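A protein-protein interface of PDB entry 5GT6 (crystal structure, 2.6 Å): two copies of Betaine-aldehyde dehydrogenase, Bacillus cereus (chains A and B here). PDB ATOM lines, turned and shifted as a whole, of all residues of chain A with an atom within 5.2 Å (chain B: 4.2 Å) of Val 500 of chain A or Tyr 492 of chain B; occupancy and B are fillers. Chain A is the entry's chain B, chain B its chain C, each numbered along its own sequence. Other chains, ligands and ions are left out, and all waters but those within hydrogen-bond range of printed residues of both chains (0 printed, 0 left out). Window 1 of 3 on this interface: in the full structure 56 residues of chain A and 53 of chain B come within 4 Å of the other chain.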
ATOM      1  N   GLY A 154      21.032 -24.856 -30.685  1.00  0.00           N
ATOM      2  CA  GLY A 154      21.830 -25.571 -29.741  1.00  0.00           C
ATOM      3  C   GLY A 154      23.253 -25.029 -29.781  1.00  0.00           C
ATOM      4  O   GLY A 154      23.528 -24.072 -30.391  1.00  0.00           O
ATOM      5  N   GLN A 155      24.148 -25.685 -29.081  1.00  0.00           N
ATOM      6  CA  GLN A 155      25.537 -25.284 -29.028  1.00  0.00           C
ATOM      7  C   GLN A 155      26.589 -26.141 -29.695  1.00  0.00           C
ATOM      8  O   GLN A 155      26.428 -27.261 -29.934  1.00  0.00           O
ATOM      9  CB  GLN A 155      25.993 -25.055 -27.584  1.00  0.00           C
ATOM     10  CG  GLN A 155      25.007 -24.482 -26.624  1.00  0.00           C
ATOM     11  CD  GLN A 155      25.509 -24.351 -25.210  1.00  0.00           C
ATOM     12  OE1 GLN A 155      26.447 -24.950 -24.815  1.00  0.00           O
ATOM     13  NE2 GLN A 155      24.865 -23.556 -24.466  1.00  0.00           N
ATOM     14  N   THR A 167      25.103 -29.817 -29.063  1.00  0.00           N
ATOM     15  CA  THR A 167      23.861 -30.123 -28.448  1.00  0.00           C
ATOM     16  C   THR A 167      22.748 -29.927 -29.437  1.00  0.00           C
ATOM     17  O   THR A 167      22.862 -29.199 -30.342  1.00  0.00           O
ATOM     18  CB  THR A 167      23.658 -29.377 -27.113  1.00  0.00           C
ATOM     19  OG1 THR A 167      23.522 -28.005 -27.331  1.00  0.00           O
ATOM     20  CG2 THR A 167      24.800 -29.546 -26.284  1.00  0.00           C
ATOM     21  N   ARG A 168      21.685 -30.661 -29.242  1.00  0.00           N
ATOM     22  CA  ARG A 168      20.523 -30.611 -30.048  1.00  0.00           C
ATOM     23  C   ARG A 168      19.401 -30.330 -29.100  1.00  0.00           C
ATOM     24  O   ARG A 168      19.355 -30.882 -28.073  1.00  0.00           O
ATOM     25  CB  ARG A 168      20.298 -31.980 -30.663  1.00  0.00           C
ATOM     26  CG  ARG A 168      20.552 -32.121 -32.127  1.00  0.00           C
ATOM     27  CD  ARG A 168      20.559 -33.562 -32.551  1.00  0.00           C
ATOM     28  NE  ARG A 168      19.248 -34.159 -32.763  1.00  0.00           N
ATOM     29  CZ  ARG A 168      18.488 -34.006 -33.824  1.00  0.00           C
ATOM     30  NH1 ARG A 168      18.855 -33.311 -34.841  1.00  0.00           N
ATOM     31  NH2 ARG A 168      17.360 -34.599 -33.882  1.00  0.00           N
ATOM     32  N   HIS A 169      18.512 -29.432 -29.452  1.00  0.00           N
ATOM     33  CA  HIS A 169      17.331 -29.128 -28.662  1.00  0.00           C
ATOM     34  C   HIS A 169      16.185 -29.828 -29.365  1.00  0.00           C
ATOM     35  O   HIS A 169      15.620 -29.320 -30.225  1.00  0.00           O
ATOM     36  CB  HIS A 169      17.133 -27.638 -28.600  1.00  0.00           C
ATOM     37  CG  HIS A 169      18.115 -26.941 -27.723  1.00  0.00           C
ATOM     38  ND1 HIS A 169      17.886 -25.705 -27.203  1.00  0.00           N
ATOM     39  CD2 HIS A 169      19.320 -27.314 -27.269  1.00  0.00           C
ATOM     40  CE1 HIS A 169      18.897 -25.351 -26.456  1.00  0.00           C
ATOM     41  NE2 HIS A 169      19.778 -26.312 -26.483  1.00  0.00           N
ATOM     42  N   GLU A 170      15.887 -31.046 -28.980  1.00  0.00           N
ATOM     43  CA  GLU A 170      14.870 -31.871 -29.661  1.00  0.00           C
ATOM     44  C   GLU A 170      13.521 -31.670 -28.947  1.00  0.00           C
ATOM     45  O   GLU A 170      13.468 -31.709 -27.710  1.00  0.00           O
ATOM     46  CB  GLU A 170      15.209 -33.367 -29.625  1.00  0.00           C
ATOM     47  CG  GLU A 170      16.649 -33.770 -29.909  1.00  0.00           C
ATOM     48  CD  GLU A 170      16.857 -35.271 -30.053  1.00  0.00           C
ATOM     49  OE1 GLU A 170      16.072 -36.058 -29.475  1.00  0.00           O
ATOM     50  OE2 GLU A 170      17.813 -35.678 -30.748  1.00  0.00           O
ATOM     51  N   THR A 498      11.538 -28.787 -24.791  1.00  0.00           N
ATOM     52  CA  THR A 498      12.710 -29.306 -25.357  1.00  0.00           C
ATOM     53  C   THR A 498      13.405 -30.295 -24.503  1.00  0.00           C
ATOM     54  O   THR A 498      13.263 -30.333 -23.342  1.00  0.00           O
ATOM     55  CB  THR A 498      13.574 -28.086 -25.765  1.00  0.00           C
ATOM     56  OG1 THR A 498      13.333 -27.800 -27.125  1.00  0.00           O
ATOM     57  CG2 THR A 498      15.036 -28.233 -25.544  1.00  0.00           C
ATOM     58  N   GLU A 499      14.178 -31.117 -25.147  1.00  0.00           N
ATOM     59  CA  GLU A 499      14.997 -32.090 -24.436  1.00  0.00           C
ATOM     60  C   GLU A 499      16.432 -31.973 -25.002  1.00  0.00           C
ATOM     61  O   GLU A 499      16.647 -32.087 -26.218  1.00  0.00           O
ATOM     62  CB  GLU A 499      14.359 -33.463 -24.595  1.00  0.00           C
ATOM     63  CG  GLU A 499      14.870 -34.532 -23.666  1.00  0.00           C
ATOM     64  CD  GLU A 499      14.249 -34.517 -22.291  1.00  0.00           C
ATOM     65  OE1 GLU A 499      13.034 -34.764 -22.165  1.00  0.00           O
ATOM     66  OE2 GLU A 499      15.027 -34.314 -21.334  1.00  0.00           O
ATOM     67  N   VAL A 500      17.384 -31.639 -24.120  1.00  0.00           N
ATOM     68  CA  VAL A 500      18.778 -31.391 -24.526  1.00  0.00           C
ATOM     69  C   VAL A 500      19.493 -32.694 -24.692  1.00  0.00           C
ATOM     70  O   VAL A 500      19.526 -33.475 -23.758  1.00  0.00           O
ATOM     71  CB  VAL A 500      19.597 -30.593 -23.503  1.00  0.00           C
ATOM     72  CG1 VAL A 500      21.060 -30.521 -23.932  1.00  0.00           C
ATOM     73  CG2 VAL A 500      19.006 -29.206 -23.350  1.00  0.00           C
ATOM     74  N   LYS A 501      20.027 -32.901 -25.895  1.00  0.00           N
ATOM     75  CA  LYS A 501      20.903 -34.005 -26.261  1.00  0.00           C
ATOM     76  C   LYS A 501      22.313 -33.446 -26.524  1.00  0.00           C
ATOM     77  O   LYS A 501      22.483 -32.508 -27.273  1.00  0.00           O
ATOM     78  CB  LYS A 501      20.365 -34.723 -27.501  1.00  0.00           C
ATOM     79  CG  LYS A 501      21.254 -35.842 -27.996  1.00  0.00           C
ATOM     80  CD  LYS A 501      20.683 -36.564 -29.173  1.00  0.00           C
ATOM     81  CE  LYS A 501      19.548 -37.477 -28.755  1.00  0.00           C
ATOM     82  NZ  LYS A 501      18.942 -38.074 -29.985  1.00  0.00           N
ATOM     83  N   SER A 502      23.305 -34.034 -25.865  1.00  0.00           N
ATOM     84  CA  SER A 502      24.722 -33.688 -26.007  1.00  0.00           C
ATOM     85  C   SER A 502      25.431 -34.792 -26.789  1.00  0.00           C
ATOM     86  O   SER A 502      25.587 -35.919 -26.295  1.00  0.00           O
ATOM     87  CB  SER A 502      25.376 -33.557 -24.643  1.00  0.00           C
ATOM     88  OG  SER A 502      26.752 -33.310 -24.789  1.00  0.00           O
ATOM     89  N   GLY B 461      20.098 -38.684 -23.274  1.00  0.00           N
ATOM     90  CA  GLY B 461      20.659 -37.377 -22.939  1.00  0.00           C
ATOM     91  C   GLY B 461      21.975 -37.055 -23.580  1.00  0.00           C
ATOM     92  O   GLY B 461      22.200 -35.924 -24.011  1.00  0.00           O
ATOM     93  N   PRO B 476      26.547 -30.472 -21.395  1.00  0.00           N
ATOM     94  CA  PRO B 476      25.439 -30.870 -20.513  1.00  0.00           C
ATOM     95  C   PRO B 476      25.281 -32.380 -20.367  1.00  0.00           C
ATOM     96  O   PRO B 476      25.536 -33.121 -21.318  1.00  0.00           O
ATOM     97  CB  PRO B 476      24.201 -30.248 -21.192  1.00  0.00           C
ATOM     98  CG  PRO B 476      24.609 -30.035 -22.620  1.00  0.00           C
ATOM     99  CD  PRO B 476      26.070 -29.689 -22.560  1.00  0.00           C
ATOM    100  N   TYR B 480      16.592 -38.424 -20.516  1.00  0.00           N
ATOM    101  CA  TYR B 480      15.263 -38.382 -21.114  1.00  0.00           C
ATOM    102  C   TYR B 480      14.438 -39.347 -20.302  1.00  0.00           C
ATOM    103  O   TYR B 480      14.989 -40.137 -19.627  1.00  0.00           O
ATOM    104  CB  TYR B 480      15.316 -38.994 -22.525  1.00  0.00           C
ATOM    105  CG  TYR B 480      15.813 -38.138 -23.637  1.00  0.00           C
ATOM    106  CD1 TYR B 480      16.959 -37.457 -23.535  1.00  0.00           C
ATOM    107  CD2 TYR B 480      15.113 -38.034 -24.798  1.00  0.00           C
ATOM    108  CE1 TYR B 480      17.391 -36.669 -24.557  1.00  0.00           C
ATOM    109  CE2 TYR B 480      15.558 -37.294 -25.826  1.00  0.00           C
ATOM    110  CZ  TYR B 480      16.682 -36.594 -25.678  1.00  0.00           C
ATOM    111  OH  TYR B 480      17.107 -35.861 -26.668  1.00  0.00           O
ATOM    112  N   ARG B 487      19.210 -30.844 -16.658  1.00  0.00           N
ATOM    113  CA  ARG B 487      20.576 -31.142 -16.971  1.00  0.00           C
ATOM    114  C   ARG B 487      21.544 -30.502 -16.029  1.00  0.00           C
ATOM    115  O   ARG B 487      21.338 -29.428 -15.573  1.00  0.00           O
ATOM    116  CB  ARG B 487      20.960 -30.676 -18.386  1.00  0.00           C
ATOM    117  CG  ARG B 487      20.190 -31.231 -19.534  1.00  0.00           C
ATOM    118  CD  ARG B 487      20.639 -32.601 -19.845  1.00  0.00           C
ATOM    119  NE  ARG B 487      19.848 -33.296 -20.830  1.00  0.00           N
ATOM    120  CZ  ARG B 487      18.699 -33.899 -20.646  1.00  0.00           C
ATOM    121  NH1 ARG B 487      18.083 -33.878 -19.521  1.00  0.00           N
ATOM    122  NH2 ARG B 487      18.166 -34.509 -21.636  1.00  0.00           N
ATOM    123  N   LEU B 489      25.887 -29.734 -15.564  1.00  0.00           N
ATOM    124  CA  LEU B 489      27.050 -29.336 -16.379  1.00  0.00           C
ATOM    125  C   LEU B 489      26.649 -28.402 -17.486  1.00  0.00           C
ATOM    126  O   LEU B 489      25.486 -28.199 -17.746  1.00  0.00           O
ATOM    127  CB  LEU B 489      27.849 -30.524 -16.932  1.00  0.00           C
ATOM    128  CG  LEU B 489      28.360 -31.533 -15.919  1.00  0.00           C
ATOM    129  CD1 LEU B 489      29.297 -32.531 -16.617  1.00  0.00           C
ATOM    130  CD2 LEU B 489      29.075 -30.843 -14.779  1.00  0.00           C
ATOM    131  N   GLY B 490      27.647 -27.797 -18.094  1.00  0.00           N
ATOM    132  CA  GLY B 490      27.466 -26.843 -19.198  1.00  0.00           C
ATOM    133  C   GLY B 490      26.817 -25.557 -18.708  1.00  0.00           C
ATOM    134  O   GLY B 490      26.681 -25.339 -17.513  1.00  0.00           O
ATOM    135  N   SER B 491      26.414 -24.730 -19.665  1.00  0.00           N
ATOM    136  CA  SER B 491      25.649 -23.533 -19.397  1.00  0.00           C
ATOM    137  C   SER B 491      24.264 -23.906 -18.851  1.00  0.00           C
ATOM    138  O   SER B 491      23.744 -23.261 -17.923  1.00  0.00           O
ATOM    139  CB  SER B 491      25.543 -22.674 -20.656  1.00  0.00           C
ATOM    140  OG  SER B 491      24.534 -23.142 -21.487  1.00  0.00           O
ATOM    141  N   TYR B 492      23.738 -25.009 -19.389  1.00  0.00           N
ATOM    142  CA  TYR B 492      22.378 -25.478 -19.099  1.00  0.00           C
ATOM    143  C   TYR B 492      22.147 -25.551 -17.606  1.00  0.00           C
ATOM    144  O   TYR B 492      21.109 -25.124 -17.136  1.00  0.00           O
ATOM    145  CB  TYR B 492      22.080 -26.845 -19.782  1.00  0.00           C
ATOM    146  CG  TYR B 492      22.129 -26.737 -21.288  1.00  0.00           C
ATOM    147  CD1 TYR B 492      23.351 -26.791 -21.976  1.00  0.00           C
ATOM    148  CD2 TYR B 492      20.968 -26.501 -22.022  1.00  0.00           C
ATOM    149  CE1 TYR B 492      23.403 -26.658 -23.342  1.00  0.00           C
ATOM    150  CE2 TYR B 492      21.010 -26.378 -23.390  1.00  0.00           C
ATOM    151  CZ  TYR B 492      22.228 -26.456 -24.051  1.00  0.00           C
ATOM    152  OH  TYR B 492      22.285 -26.313 -25.416  1.00  0.00           O
ATOM    153  N   ALA B 493      23.127 -26.039 -16.852  1.00  0.00           N
ATOM    154  CA  ALA B 493      22.951 -26.242 -15.433  1.00  0.00           C
ATOM    155  C   ALA B 493      22.618 -24.973 -14.655  1.00  0.00           C
ATOM    156  O   ALA B 493      21.973 -25.052 -13.638  1.00  0.00           O
ATOM    157  CB  ALA B 493      24.174 -26.909 -14.850  1.00  0.00           C
ATOM    158  N   LEU B 494      23.018 -23.812 -15.140  1.00  0.00           N
ATOM    159  CA  LEU B 494      22.798 -22.550 -14.412  1.00  0.00           C
ATOM    160  C   LEU B 494      21.327 -22.263 -14.242  1.00  0.00           C
ATOM    161  O   LEU B 494      20.917 -21.740 -13.200  1.00  0.00           O
ATOM    162  CB  LEU B 494      23.450 -21.373 -15.159  1.00  0.00           C
ATOM    163  CG  LEU B 494      24.971 -21.494 -15.318  1.00  0.00           C
ATOM    164  CD1 LEU B 494      25.506 -20.552 -16.378  1.00  0.00           C
ATOM    165  CD2 LEU B 494      25.648 -21.266 -13.976  1.00  0.00           C
ATOM    166  N   ASP B 495      20.551 -22.644 -15.260  1.00  0.00           N
ATOM    167  CA  ASP B 495      19.096 -22.422 -15.296  1.00  0.00           C
ATOM    168  C   ASP B 495      18.348 -23.081 -14.148  1.00  0.00           C
ATOM    169  O   ASP B 495      17.350 -22.538 -13.685  1.00  0.00           O
ATOM    170  CB  ASP B 495      18.466 -22.878 -16.641  1.00  0.00           C
ATOM    171  CG  ASP B 495      19.087 -22.173 -17.871  1.00  0.00           C
ATOM    172  OD1 ASP B 495      19.913 -21.234 -17.722  1.00  0.00           O
ATOM    173  OD2 ASP B 495      18.759 -22.585 -19.009  1.00  0.00           O
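The side-chain hydroxyl of Ser 491 of chain B is in hydrogen-bond range of the side-chain amide nitrogen of Gln 155 of chain A (3.0 Å). OG1 of Thr 167 of chain A lies within hydrogen-bond range of OH of Tyr 492 of chain B (2.8 Å). NE2 of His 169 of chain A sits at hydrogen-bond distance from OH of Tyr 492 of chain B (2.7 Å). OE1 of Glu 170 of chain A is in hydrogen-bond range of OH of Tyr 480 of chain B (3.0 Å). OE2 of Glu 499 of chain A is in salt-bridge range of NH2 of Arg 487 of chain B (3.2 Å). The backbone carbonyl oxygen (O) of Val 500 of chain A lies within hydrogen-bond range of the guanidinium group (NH2) of Arg 487 of chain B (2.7 Å). N of Ser 502 of chain A is in hydrogen-bond range of O of Gly 461 of chain B (2.9 Å).
The side-chain hydroxyl (OG1) of Thr 167 of chain A is in hydrogen-bond range of the backbone NH (N) of Gln 155 of chain A. OE2 of Glu 170 of chain A is in salt-bridge range of NE of Arg 168 of chain A (2.9 Å). N of Arg 168 of chain A lies within hydrogen-bond range of O of Lys 501 of chain A, at 2.8 Å. O of Glu 170 of chain A is in hydrogen-bond range of N of Glu 499 of chain A (2.7 Å). The side-chain amino group (NZ) of Lys 501 of chain A is in salt-bridge range of the side-chain carboxylate (OE2) of Glu 170 of chain A.
Among the printed residues, merely in contact across the chains: Gln 155 of chain A with Tyr 492 of chain B (3.5 Å), Thr 167 of chain A with Pro 476 of chain B (3.7 Å), Glu 499 of chain A with Tyr 480 of chain B (3.4 Å), Val 500 of chain A with Gly 461 of chain B (3.6 Å), Val 500 of chain A with Pro 476 of chain B (3.8 Å), Val 500 of chain A with Tyr 480 of chain B (3.9 Å), Val 500 of chain A with Tyr 492 of chain B (3.5 Å), Lys 501 of chain A with Gly 461 of chain B (3.2 Å), Lys 501 of chain A with Tyr 480 of chain B (3.6 Å) and Ser 502 of chain A with Pro 476 of chain B (3.4 Å).
Of the printed residues of chain B, Thr 167 of chain A touches Pro 476 (3.7 Å) and Tyr 492 (2.8 Å). Of the printed residues of chain B, Glu 170 of chain A touches Tyr 480. Val 500 of chain A touches just these residues of chain B: Gly 461, Pro 476, Tyr 480, Arg 487 and Tyr 492. Of the printed residues of chain B, Lys 501 of chain A touches Gly 461 and Tyr 480. Printed residues of chain A within 4 Å of Gly 461 of chain B: Val 500 (3.6 Å), Lys 501 (3.2 Å) and Ser 502 (2.9 Å). Of the printed residues of chain A, Tyr 480 of chain B touches Glu 170, Glu 499, Val 500 and Lys 501. Tyr 492 of chain B touches just these residues of chain A: Gln 155 (3.5 Å), Thr 167 (2.8 Å), His 169 (2.7 Å) and Val 500 (3.5 Å). The nearest printed residue of chain B that does not touch Thr 167 of chain A is Gly 461 of chain B (7.3 Å).
Of the 11 printed residues of chain B, 6 touch a printed residue of chain A. Along chain B the printed residues that touch a printed residue of chain A span positions 461 to 492. Of the 11 printed residues of chain A, 8 touch a printed residue of chain B. Printed residues of chain A that touch a printed residue of chain B: Gln 155, Thr 167, His 169, Glu 170, Glu 499, Val 500, Lys 501 and Ser 502. Hydrophobic or aromatic side chains of chain A that line the printed part of chain B: His 169 and Val 500.
No position is printed for both chains.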
